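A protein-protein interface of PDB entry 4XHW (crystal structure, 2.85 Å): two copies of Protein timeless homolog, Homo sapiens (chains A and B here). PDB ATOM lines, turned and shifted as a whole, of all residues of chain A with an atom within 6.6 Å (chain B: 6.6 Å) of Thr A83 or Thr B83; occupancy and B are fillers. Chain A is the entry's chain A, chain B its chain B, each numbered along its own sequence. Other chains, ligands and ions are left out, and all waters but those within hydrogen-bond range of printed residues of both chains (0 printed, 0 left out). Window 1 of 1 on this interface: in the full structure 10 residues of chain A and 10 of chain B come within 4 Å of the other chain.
Of the printed residues of chain B, Glu A61 touches Gln B81 (3.7 Å), Glu B82 (3.2 Å) and Thr B83 (3.0 Å). Thr A83 touches just these residues of chain B: Glu B57, Glu B61 and Thr B83. Printed residues of chain B within 4 Å of Arg A86: Glu B57. Leu B49 touches none of the printed residues of chain A. Printed residues of chain A within 4 Å of Glu B58: Gln A81 (3.7 Å). Pro B77 touches none of the printed residues of chain A. Of the printed residues of chain A, Thr B83 touches Glu A57, Glu A61 and Thr A83. The nearest residue of chain B that does not touch Thr A83 is Pro B51 (4.2 Å). The nearest residue of chain A that does not touch Thr B83 is Pro A51 (4.5 Å). The nearest printed residue of chain B that does not touch Phe A84 is Thr B83 (4.6 Å).
N of Ala A78 sits at hydrogen-bond distance from OE1 of Glu A82 (3.1 Å). The guanidinium group (NE) of Arg A86 is in salt-bridge range of the side-chain carboxylate (OE2) of Glu A82. O of Phe A84 sits at hydrogen-bond distance from NH1 of Arg A86 (2.7 Å). N of Ala B78 sits at hydrogen-bond distance from OE1 of Glu B82, 2.8 Å away. OE2 of Glu B82 is in salt-bridge range of NE of Arg B86 (3.7 Å). The guanidinium group of Arg B86 lies within hydrogen-bond range of the backbone carbonyl oxygen of Phe B84.
Hydrophobic or aromatic side chains of chain B within 4 Å of the printed part of chain A: Phe B84. Of the 15 printed residues of chain A, 9 touch a printed residue of chain B.
Glu A57 touches Thr B83, and with the chains exchanged Thr A83 touches Glu B57. Glu A57 touches Phe B84, and with the chains exchanged Phe A84 touches Glu B57. Glu A58 touches Gln B81, and with the chains exchanged Gln A81 touches Glu B58. Phe B84 touches its own counterpart, Phe A84. Positions printed for both chains: 49, 51, 56, 57, 58, 60, 61, 77, 78, 81, 82, 83, 84, 85 and 86. Of the 20 pairs that touch across the chains among the printed residues, 18 have their exchanged pair printed and touching as well.
O of Pro A51 touches CE2 of Phe B84, at 3.1 Å. O of Glu A57 touches O of Gln B81, 3.9 Å away. CA of Glu B82 touches OE2 of Glu A57, at 3.5 Å. CA of Glu A58 touches O of Gln B81 (3.4 Å). Glu A61 touches Gln B81 (CB to N, 3.7 Å). O of Glu B82 touches CG of Glu A61 (3.2 Å). Glu B58 touches Gln A81 (CA to O, 3.7 Å). Glu A82 touches Glu B57 (C to OE2, 3.5 Å). Glu A82 touches Glu B61. Phe A84 touches Phe B84.
The backbone NH (N) of Thr B83 sits at hydrogen-bond distance from the side-chain carboxylate (OE2) of Glu A57 (2.6 Å). The side-chain carboxylate of Glu A57 sits at hydrogen-bond distance from the backbone NH of Phe B84, at 2.9 Å. The guanidinium group (NH1) of Arg B86 lies within salt-bridge range of the side-chain carboxylate (OE2) of Glu A57, 2.6 Å away. OE2 of Glu A61 is in hydrogen-bond range of OG1 of Thr B83, at 3.0 Å. N of Thr A83 lies within hydrogen-bond range of OE2 of Glu B57. OE2 of Glu B61 sits at hydrogen-bond distance from OG1 of Thr A83, at 3.0 Å. The backbone NH (N) of Phe A84 is in hydrogen-bond range of the side-chain carboxylate (OE2) of Glu B57 (3.1 Å). OE1 of Glu B57 is in salt-bridge range of NH2 of Arg A86 (2.6 Å).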
ATOM      1  N   LEU A  49      -4.136   7.497   2.866  1.00  0.00           N
ATOM      2  CA  LEU A  49      -5.516   7.935   2.766  1.00  0.00           C
ATOM      3  C   LEU A  49      -6.179   7.086   1.721  1.00  0.00           C
ATOM      4  O   LEU A  49      -5.928   7.268   0.518  1.00  0.00           O
ATOM      5  CB  LEU A  49      -5.652   9.390   2.378  1.00  0.00           C
ATOM      6  CG  LEU A  49      -5.394  10.482   3.394  1.00  0.00           C
ATOM      7  CD1 LEU A  49      -5.639  11.849   2.725  1.00  0.00           C
ATOM      8  CD2 LEU A  49      -6.363  10.244   4.522  1.00  0.00           C
ATOM      9  N   PRO A  51      -9.502   6.156   0.022  1.00  0.00           N
ATOM     10  CA  PRO A  51     -10.883   6.480  -0.338  1.00  0.00           C
ATOM     11  C   PRO A  51     -11.665   5.243  -0.732  1.00  0.00           C
ATOM     12  O   PRO A  51     -11.257   4.566  -1.667  1.00  0.00           O
ATOM     13  CB  PRO A  51     -10.717   7.413  -1.531  1.00  0.00           C
ATOM     14  CG  PRO A  51      -9.422   7.030  -2.110  1.00  0.00           C
ATOM     15  CD  PRO A  51      -8.547   6.600  -0.997  1.00  0.00           C
ATOM     16  N   ASN A  56     -15.530  10.198  -2.069  1.00  0.00           N
ATOM     17  CA  ASN A  56     -14.199  10.445  -1.515  1.00  0.00           C
ATOM     18  C   ASN A  56     -13.127  10.279  -2.566  1.00  0.00           C
ATOM     19  O   ASN A  56     -12.097  10.936  -2.559  1.00  0.00           O
ATOM     20  CB  ASN A  56     -13.880   9.488  -0.380  1.00  0.00           C
ATOM     21  CG  ASN A  56     -14.819   9.625   0.764  1.00  0.00           C
ATOM     22  OD1 ASN A  56     -15.834  10.306   0.662  1.00  0.00           O
ATOM     23  ND2 ASN A  56     -14.481   8.996   1.882  1.00  0.00           N
ATOM     24  N   GLU A  57     -13.360   9.314  -3.433  1.00  0.00           N
ATOM     25  CA  GLU A  57     -12.482   9.057  -4.547  1.00  0.00           C
ATOM     26  C   GLU A  57     -12.484  10.298  -5.433  1.00  0.00           C
ATOM     27  O   GLU A  57     -11.438  10.783  -5.860  1.00  0.00           O
ATOM     28  CB  GLU A  57     -12.937   7.790  -5.247  1.00  0.00           C
ATOM     29  CG  GLU A  57     -11.944   7.193  -6.165  1.00  0.00           C
ATOM     30  CD  GLU A  57     -12.512   6.005  -6.871  1.00  0.00           C
ATOM     31  OE1 GLU A  57     -13.591   5.523  -6.455  1.00  0.00           O
ATOM     32  OE2 GLU A  57     -11.878   5.549  -7.834  1.00  0.00           O
ATOM     33  N   GLU A  58     -13.680  10.816  -5.687  1.00  0.00           N
ATOM     34  CA  GLU A  58     -13.823  12.018  -6.484  1.00  0.00           C
ATOM     35  C   GLU A  58     -13.029  13.154  -5.888  1.00  0.00           C
ATOM     36  O   GLU A  58     -12.371  13.892  -6.614  1.00  0.00           O
ATOM     37  CB  GLU A  58     -15.279  12.459  -6.553  1.00  0.00           C
ATOM     38  CG  GLU A  58     -15.525  13.533  -7.587  1.00  0.00           C
ATOM     39  CD  GLU A  58     -16.842  14.253  -7.378  1.00  0.00           C
ATOM     40  OE1 GLU A  58     -17.850  13.580  -7.065  1.00  0.00           O
ATOM     41  OE2 GLU A  58     -16.849  15.506  -7.495  1.00  0.00           O
ATOM     42  N   MET A  60     -10.225  13.144  -3.771  1.00  0.00           N
ATOM     43  CA  MET A  60      -8.790  12.959  -4.005  1.00  0.00           C
ATOM     44  C   MET A  60      -8.322  13.275  -5.429  1.00  0.00           C
ATOM     45  O   MET A  60      -7.133  13.485  -5.662  1.00  0.00           O
ATOM     46  CB  MET A  60      -8.399  11.527  -3.669  1.00  0.00           C
ATOM     47  CG  MET A  60      -8.889  11.100  -2.315  1.00  0.00           C
ATOM     48  SD  MET A  60      -7.863  11.878  -0.848  1.00  0.00           S
ATOM     49  CE  MET A  60      -6.073  11.418  -1.456  1.00  0.00           C
ATOM     50  N   GLU A  61      -9.232  13.283  -6.395  1.00  0.00           N
ATOM     51  CA  GLU A  61      -8.800  13.510  -7.748  1.00  0.00           C
ATOM     52  C   GLU A  61      -9.089  14.919  -8.174  1.00  0.00           C
ATOM     53  O   GLU A  61      -8.889  15.287  -9.335  1.00  0.00           O
ATOM     54  CB  GLU A  61      -9.474  12.531  -8.680  1.00  0.00           C
ATOM     55  CG  GLU A  61      -9.110  11.104  -8.413  1.00  0.00           C
ATOM     56  CD  GLU A  61      -7.623  10.889  -8.465  1.00  0.00           C
ATOM     57  OE1 GLU A  61      -6.931  11.586  -9.243  1.00  0.00           O
ATOM     58  OE2 GLU A  61      -7.154   9.987  -7.753  1.00  0.00           O
ATOM     59  N   PRO A  77       1.119  10.574  -3.468  1.00  0.00           N
ATOM     60  CA  PRO A  77       1.750   9.266  -3.580  1.00  0.00           C
ATOM     61  C   PRO A  77       2.985   9.328  -4.457  1.00  0.00           C
ATOM     62  O   PRO A  77       3.053  10.146  -5.386  1.00  0.00           O
ATOM     63  CB  PRO A  77       0.663   8.405  -4.213  1.00  0.00           C
ATOM     64  CG  PRO A  77      -0.241   9.334  -4.875  1.00  0.00           C
ATOM     65  CD  PRO A  77      -0.171  10.636  -4.173  1.00  0.00           C
ATOM     66  N   ALA A  78       3.948   8.470  -4.132  1.00  0.00           N
ATOM     67  CA  ALA A  78       5.158   8.256  -4.920  1.00  0.00           C
ATOM     68  C   ALA A  78       4.847   7.625  -6.284  1.00  0.00           C
ATOM     69  O   ALA A  78       4.317   6.515  -6.343  1.00  0.00           O
ATOM     70  CB  ALA A  78       6.133   7.367  -4.141  1.00  0.00           C
ATOM     71  N   GLN A  81       5.119   3.717  -7.523  1.00  0.00           N
ATOM     72  CA  GLN A  81       5.256   2.804  -6.405  1.00  0.00           C
ATOM     73  C   GLN A  81       4.029   2.831  -5.483  1.00  0.00           C
ATOM     74  O   GLN A  81       3.688   1.812  -4.889  1.00  0.00           O
ATOM     75  CB  GLN A  81       6.568   3.097  -5.680  1.00  0.00           C
ATOM     76  CG  GLN A  81       7.080   1.925  -4.848  1.00  0.00           C
ATOM     77  CD  GLN A  81       8.610   1.856  -4.814  1.00  0.00           C
ATOM     78  OE1 GLN A  81       9.295   2.878  -4.727  1.00  0.00           O
ATOM     79  NE2 GLN A  81       9.149   0.636  -4.894  1.00  0.00           N
ATOM     80  N   GLU A  82       3.356   3.979  -5.381  1.00  0.00           N
ATOM     81  CA  GLU A  82       2.133   4.106  -4.561  1.00  0.00           C
ATOM     82  C   GLU A  82       0.878   4.588  -5.309  1.00  0.00           C
ATOM     83  O   GLU A  82       0.951   5.218  -6.365  1.00  0.00           O
ATOM     84  CB  GLU A  82       2.367   5.045  -3.378  1.00  0.00           C
ATOM     85  CG  GLU A  82       3.179   4.453  -2.255  1.00  0.00           C
ATOM     86  CD  GLU A  82       3.668   5.489  -1.274  1.00  0.00           C
ATOM     87  OE1 GLU A  82       3.729   6.680  -1.657  1.00  0.00           O
ATOM     88  OE2 GLU A  82       3.956   5.113  -0.116  1.00  0.00           O
ATOM     89  N   THR A  83      -0.279   4.284  -4.741  1.00  0.00           N
ATOM     90  CA  THR A  83      -1.551   4.772  -5.262  1.00  0.00           C
ATOM     91  C   THR A  83      -2.103   5.881  -4.364  1.00  0.00           C
ATOM     92  O   THR A  83      -2.646   6.871  -4.837  1.00  0.00           O
ATOM     93  CB  THR A  83      -2.593   3.651  -5.349  1.00  0.00           C
ATOM     94  OG1 THR A  83      -2.101   2.598  -6.186  1.00  0.00           O
ATOM     95  CG2 THR A  83      -3.902   4.176  -5.892  1.00  0.00           C
ATOM     96  N   PHE A  84      -1.949   5.713  -3.060  1.00  0.00           N
ATOM     97  CA  PHE A  84      -2.598   6.586  -2.112  1.00  0.00           C
ATOM     98  C   PHE A  84      -1.704   7.709  -1.578  1.00  0.00           C
ATOM     99  O   PHE A  84      -0.489   7.561  -1.476  1.00  0.00           O
ATOM    100  CB  PHE A  84      -3.123   5.756  -0.960  1.00  0.00           C
ATOM    101  CG  PHE A  84      -4.075   4.693  -1.382  1.00  0.00           C
ATOM    102  CD1 PHE A  84      -5.182   5.012  -2.143  1.00  0.00           C
ATOM    103  CD2 PHE A  84      -3.868   3.363  -1.014  1.00  0.00           C
ATOM    104  CE1 PHE A  84      -6.085   4.019  -2.520  1.00  0.00           C
ATOM    105  CE2 PHE A  84      -4.754   2.369  -1.387  1.00  0.00           C
ATOM    106  CZ  PHE A  84      -5.862   2.691  -2.146  1.00  0.00           C
ATOM    107  N   TRP A  85      -2.319   8.842  -1.247  1.00  0.00           N
ATOM    108  CA  TRP A  85      -1.597   9.866  -0.509  1.00  0.00           C
ATOM    109  C   TRP A  85      -1.302   9.278   0.842  1.00  0.00           C
ATOM    110  O   TRP A  85      -1.998   8.366   1.303  1.00  0.00           O
ATOM    111  CB  TRP A  85      -2.393  11.164  -0.354  1.00  0.00           C
ATOM    112  CG  TRP A  85      -2.580  11.911  -1.638  1.00  0.00           C
ATOM    113  CD1 TRP A  85      -3.117  11.430  -2.785  1.00  0.00           C
ATOM    114  CD2 TRP A  85      -2.242  13.289  -1.898  1.00  0.00           C
ATOM    115  NE1 TRP A  85      -3.133  12.411  -3.747  1.00  0.00           N
ATOM    116  CE2 TRP A  85      -2.604  13.546  -3.231  1.00  0.00           C
ATOM    117  CE3 TRP A  85      -1.672  14.304  -1.136  1.00  0.00           C
ATOM    118  CZ2 TRP A  85      -2.405  14.797  -3.812  1.00  0.00           C
ATOM    119  CZ3 TRP A  85      -1.472  15.540  -1.726  1.00  0.00           C
ATOM    120  CH2 TRP A  85      -1.843  15.775  -3.049  1.00  0.00           C
ATOM    121  N   ARG A  86      -0.282   9.828   1.480  1.00  0.00           N
ATOM    122  CA  ARG A  86       0.108   9.394   2.795  1.00  0.00           C
ATOM    123  C   ARG A  86       0.038  10.524   3.788  1.00  0.00           C
ATOM    124  O   ARG A  86       0.452  11.643   3.499  1.00  0.00           O
ATOM    125  CB  ARG A  86       1.523   8.808   2.752  1.00  0.00           C
ATOM    126  CG  ARG A  86       1.548   7.301   2.715  1.00  0.00           C
ATOM    127  CD  ARG A  86       1.198   6.727   1.371  1.00  0.00           C
ATOM    128  NE  ARG A  86       1.144   5.270   1.424  1.00  0.00           N
ATOM    129  CZ  ARG A  86       0.710   4.501   0.428  1.00  0.00           C
ATOM    130  NH1 ARG A  86       0.281   5.051  -0.698  1.00  0.00           N
ATOM    131  NH2 ARG A  86       0.685   3.176   0.562  1.00  0.00           N
ATOM    132  N   LEU B  49     -11.188  -1.818  -8.570  1.00  0.00           N
ATOM    133  CA  LEU B  49     -10.100  -2.622  -8.054  1.00  0.00           C
ATOM    134  C   LEU B  49      -9.412  -1.765  -7.028  1.00  0.00           C
ATOM    135  O   LEU B  49      -8.590  -0.931  -7.369  1.00  0.00           O
ATOM    136  CB  LEU B  49      -9.144  -3.019  -9.178  1.00  0.00           C
ATOM    137  CG  LEU B  49      -9.735  -3.958 -10.250  1.00  0.00           C
ATOM    138  CD1 LEU B  49      -8.689  -4.302 -11.298  1.00  0.00           C
ATOM    139  CD2 LEU B  49     -10.382  -5.215  -9.669  1.00  0.00           C
ATOM    140  N   PRO B  51      -6.768  -1.496  -4.256  1.00  0.00           N
ATOM    141  CA  PRO B  51      -5.622  -2.125  -3.573  1.00  0.00           C
ATOM    142  C   PRO B  51      -5.622  -1.768  -2.085  1.00  0.00           C
ATOM    143  O   PRO B  51      -5.600  -0.602  -1.750  1.00  0.00           O
ATOM    144  CB  PRO B  51      -4.404  -1.521  -4.279  1.00  0.00           C
ATOM    145  CG  PRO B  51      -4.897  -0.179  -4.770  1.00  0.00           C
ATOM    146  CD  PRO B  51      -6.360  -0.370  -5.120  1.00  0.00           C
ATOM    147  N   ASN B  56      -0.442  -4.889  -3.393  1.00  0.00           N
ATOM    148  CA  ASN B  56      -1.442  -4.719  -4.436  1.00  0.00           C
ATOM    149  C   ASN B  56      -1.368  -3.310  -5.016  1.00  0.00           C
ATOM    150  O   ASN B  56      -1.627  -3.095  -6.192  1.00  0.00           O
ATOM    151  CB  ASN B  56      -2.839  -4.995  -3.901  1.00  0.00           C
ATOM    152  CG  ASN B  56      -3.036  -6.425  -3.541  1.00  0.00           C
ATOM    153  OD1 ASN B  56      -2.094  -7.199  -3.574  1.00  0.00           O
ATOM    154  ND2 ASN B  56      -4.260  -6.794  -3.188  1.00  0.00           N
ATOM    155  N   GLU B  57      -1.043  -2.352  -4.159  1.00  0.00           N
ATOM    156  CA  GLU B  57      -0.828  -0.991  -4.582  1.00  0.00           C
ATOM    157  C   GLU B  57       0.305  -0.944  -5.580  1.00  0.00           C
ATOM    158  O   GLU B  57       0.158  -0.457  -6.724  1.00  0.00           O
ATOM    159  CB  GLU B  57      -0.499  -0.146  -3.374  1.00  0.00           C
ATOM    160  CG  GLU B  57      -1.524   0.899  -3.050  1.00  0.00           C
ATOM    161  CD  GLU B  57      -1.002   1.930  -2.057  1.00  0.00           C
ATOM    162  OE1 GLU B  57      -0.951   1.624  -0.824  1.00  0.00           O
ATOM    163  OE2 GLU B  57      -0.598   3.015  -2.540  1.00  0.00           O
ATOM    164  N   GLU B  58       1.415  -1.546  -5.162  1.00  0.00           N
ATOM    165  CA  GLU B  58       2.629  -1.573  -5.946  1.00  0.00           C
ATOM    166  C   GLU B  58       2.290  -2.181  -7.292  1.00  0.00           C
ATOM    167  O   GLU B  58       2.755  -1.715  -8.334  1.00  0.00           O
ATOM    168  CB  GLU B  58       3.711  -2.388  -5.243  1.00  0.00           C
ATOM    169  CG  GLU B  58       5.133  -2.128  -5.726  1.00  0.00           C
ATOM    170  CD  GLU B  58       6.103  -3.219  -5.295  1.00  0.00           C
ATOM    171  OE1 GLU B  58       5.980  -3.722  -4.156  1.00  0.00           O
ATOM    172  OE2 GLU B  58       7.014  -3.548  -6.087  1.00  0.00           O
ATOM    173  N   MET B  60      -0.739  -2.245  -8.802  1.00  0.00           N
ATOM    174  CA  MET B  60      -1.570  -1.359  -9.592  1.00  0.00           C
ATOM    175  C   MET B  60      -0.813  -0.189 -10.161  1.00  0.00           C
ATOM    176  O   MET B  60      -1.374   0.590 -10.938  1.00  0.00           O
ATOM    177  CB  MET B  60      -2.727  -0.812  -8.791  1.00  0.00           C
ATOM    178  CG  MET B  60      -3.914  -0.601  -9.691  1.00  0.00           C
ATOM    179  SD  MET B  60      -4.655  -2.357  -9.843  1.00  0.00           S
ATOM    180  CE  MET B  60      -4.737  -2.470  -7.936  1.00  0.00           C
ATOM    181  N   GLU B  61       0.441  -0.031  -9.746  1.00  0.00           N
ATOM    182  CA  GLU B  61       1.254   1.024 -10.339  1.00  0.00           C
ATOM    183  C   GLU B  61       2.329   0.449 -11.262  1.00  0.00           C
ATOM    184  O   GLU B  61       3.183   1.174 -11.770  1.00  0.00           O
ATOM    185  CB  GLU B  61       1.864   1.892  -9.250  1.00  0.00           C
ATOM    186  CG  GLU B  61       0.811   2.586  -8.419  1.00  0.00           C
ATOM    187  CD  GLU B  61      -0.128   3.460  -9.241  1.00  0.00           C
ATOM    188  OE1 GLU B  61       0.333   4.105 -10.218  1.00  0.00           O
ATOM    189  OE2 GLU B  61      -1.344   3.474  -8.930  1.00  0.00           O
ATOM    190  N   PRO B  77      -8.971   4.297 -14.606  1.00  0.00           N
ATOM    191  CA  PRO B  77      -9.853   5.261 -13.948  1.00  0.00           C
ATOM    192  C   PRO B  77     -10.021   6.505 -14.786  1.00  0.00           C
ATOM    193  O   PRO B  77      -9.161   6.810 -15.620  1.00  0.00           O
ATOM    194  CB  PRO B  77      -9.145   5.551 -12.623  1.00  0.00           C
ATOM    195  CG  PRO B  77      -7.745   5.163 -12.837  1.00  0.00           C
ATOM    196  CD  PRO B  77      -7.702   4.110 -13.885  1.00  0.00           C
ATOM    197  N   ALA B  78     -11.173   7.147 -14.637  1.00  0.00           N
ATOM    198  CA  ALA B  78     -11.421   8.429 -15.264  1.00  0.00           C
ATOM    199  C   ALA B  78     -10.521   9.474 -14.618  1.00  0.00           C
ATOM    200  O   ALA B  78     -10.671   9.790 -13.441  1.00  0.00           O
ATOM    201  CB  ALA B  78     -12.865   8.808 -15.117  1.00  0.00           C
ATOM    202  N   GLN B  81     -11.517  12.065 -11.752  1.00  0.00           N
ATOM    203  CA  GLN B  81     -12.722  11.618 -11.056  1.00  0.00           C
ATOM    204  C   GLN B  81     -12.565  10.336 -10.265  1.00  0.00           C
ATOM    205  O   GLN B  81     -13.211  10.150  -9.233  1.00  0.00           O
ATOM    206  CB  GLN B  81     -13.863  11.453 -12.049  1.00  0.00           C
ATOM    207  CG  GLN B  81     -14.119  12.727 -12.765  1.00  0.00           C
ATOM    208  CD  GLN B  81     -14.991  13.657 -11.930  1.00  0.00           C
ATOM    209  OE1 GLN B  81     -15.763  13.197 -11.073  1.00  0.00           O
ATOM    210  NE2 GLN B  81     -14.798  14.969 -12.101  1.00  0.00           N
ATOM    211  N   GLU B  82     -11.728   9.442 -10.768  1.00  0.00           N
ATOM    212  CA  GLU B  82     -11.553   8.166 -10.146  1.00  0.00           C
ATOM    213  C   GLU B  82     -10.113   7.909  -9.802  1.00  0.00           C
ATOM    214  O   GLU B  82      -9.210   8.511 -10.368  1.00  0.00           O
ATOM    215  CB  GLU B  82     -12.068   7.075 -11.062  1.00  0.00           C
ATOM    216  CG  GLU B  82     -13.551   7.056 -11.169  1.00  0.00           C
ATOM    217  CD  GLU B  82     -14.039   6.192 -12.293  1.00  0.00           C
ATOM    218  OE1 GLU B  82     -13.240   5.879 -13.205  1.00  0.00           O
ATOM    219  OE2 GLU B  82     -15.238   5.857 -12.271  1.00  0.00           O
ATOM    220  N   THR B  83      -9.919   7.004  -8.862  1.00  0.00           N
ATOM    221  CA  THR B  83      -8.613   6.537  -8.470  1.00  0.00           C
ATOM    222  C   THR B  83      -8.365   5.132  -8.975  1.00  0.00           C
ATOM    223  O   THR B  83      -7.272   4.790  -9.420  1.00  0.00           O
ATOM    224  CB  THR B  83      -8.489   6.531  -6.954  1.00  0.00           C
ATOM    225  OG1 THR B  83      -8.736   7.855  -6.454  1.00  0.00           O
ATOM    226  CG2 THR B  83      -7.117   6.045  -6.542  1.00  0.00           C
ATOM    227  N   PHE B  84      -9.417   4.331  -8.899  1.00  0.00           N
ATOM    228  CA  PHE B  84      -9.342   2.891  -9.095  1.00  0.00           C
ATOM    229  C   PHE B  84      -9.753   2.498 -10.505  1.00  0.00           C
ATOM    230  O   PHE B  84     -10.618   3.150 -11.105  1.00  0.00           O
ATOM    231  CB  PHE B  84     -10.252   2.191  -8.085  1.00  0.00           C
ATOM    232  CG  PHE B  84      -9.996   2.596  -6.653  1.00  0.00           C
ATOM    233  CD1 PHE B  84      -8.718   2.643  -6.149  1.00  0.00           C
ATOM    234  CD2 PHE B  84     -11.047   2.950  -5.820  1.00  0.00           C
ATOM    235  CE1 PHE B  84      -8.486   3.037  -4.825  1.00  0.00           C
ATOM    236  CE2 PHE B  84     -10.834   3.332  -4.513  1.00  0.00           C
ATOM    237  CZ  PHE B  84      -9.550   3.383  -4.011  1.00  0.00           C
ATOM    238  N   TRP B  85      -9.140   1.429 -11.016  1.00  0.00           N
ATOM    239  CA  TRP B  85      -9.589   0.803 -12.250  1.00  0.00           C
ATOM    240  C   TRP B  85     -10.927   0.158 -12.020  1.00  0.00           C
ATOM    241  O   TRP B  85     -11.226  -0.224 -10.900  1.00  0.00           O
ATOM    242  CB  TRP B  85      -8.596  -0.245 -12.705  1.00  0.00           C
ATOM    243  CG  TRP B  85      -7.332   0.346 -13.160  1.00  0.00           C
ATOM    244  CD1 TRP B  85      -6.511   1.178 -12.455  1.00  0.00           C
ATOM    245  CD2 TRP B  85      -6.740   0.190 -14.448  1.00  0.00           C
ATOM    246  NE1 TRP B  85      -5.432   1.535 -13.220  1.00  0.00           N
ATOM    247  CE2 TRP B  85      -5.559   0.954 -14.457  1.00  0.00           C
ATOM    248  CE3 TRP B  85      -7.094  -0.525 -15.592  1.00  0.00           C
ATOM    249  CZ2 TRP B  85      -4.725   1.019 -15.578  1.00  0.00           C
ATOM    250  CZ3 TRP B  85      -6.269  -0.447 -16.700  1.00  0.00           C
ATOM    251  CH2 TRP B  85      -5.098   0.315 -16.681  1.00  0.00           C
ATOM    252  N   ARG B  86     -11.725  -0.008 -13.066  1.00  0.00           N
ATOM    253  CA  ARG B  86     -13.014  -0.690 -12.923  1.00  0.00           C
ATOM    254  C   ARG B  86     -13.193  -1.897 -13.824  1.00  0.00           C
ATOM    255  O   ARG B  86     -12.806  -1.888 -14.992  1.00  0.00           O
ATOM    256  CB  ARG B  86     -14.188   0.258 -13.184  1.00  0.00           C
ATOM    257  CG  ARG B  86     -14.747   1.007 -11.985  1.00  0.00           C
ATOM    258  CD  ARG B  86     -13.959   2.226 -11.479  1.00  0.00           C
ATOM    259  NE  ARG B  86     -14.622   2.769 -10.278  1.00  0.00           N
ATOM    260  CZ  ARG B  86     -14.119   3.714  -9.488  1.00  0.00           C
ATOM    261  NH1 ARG B  86     -12.921   4.218  -9.749  1.00  0.00           N
ATOM    262  NH2 ARG B  86     -14.807   4.136  -8.431  1.00  0.00           N
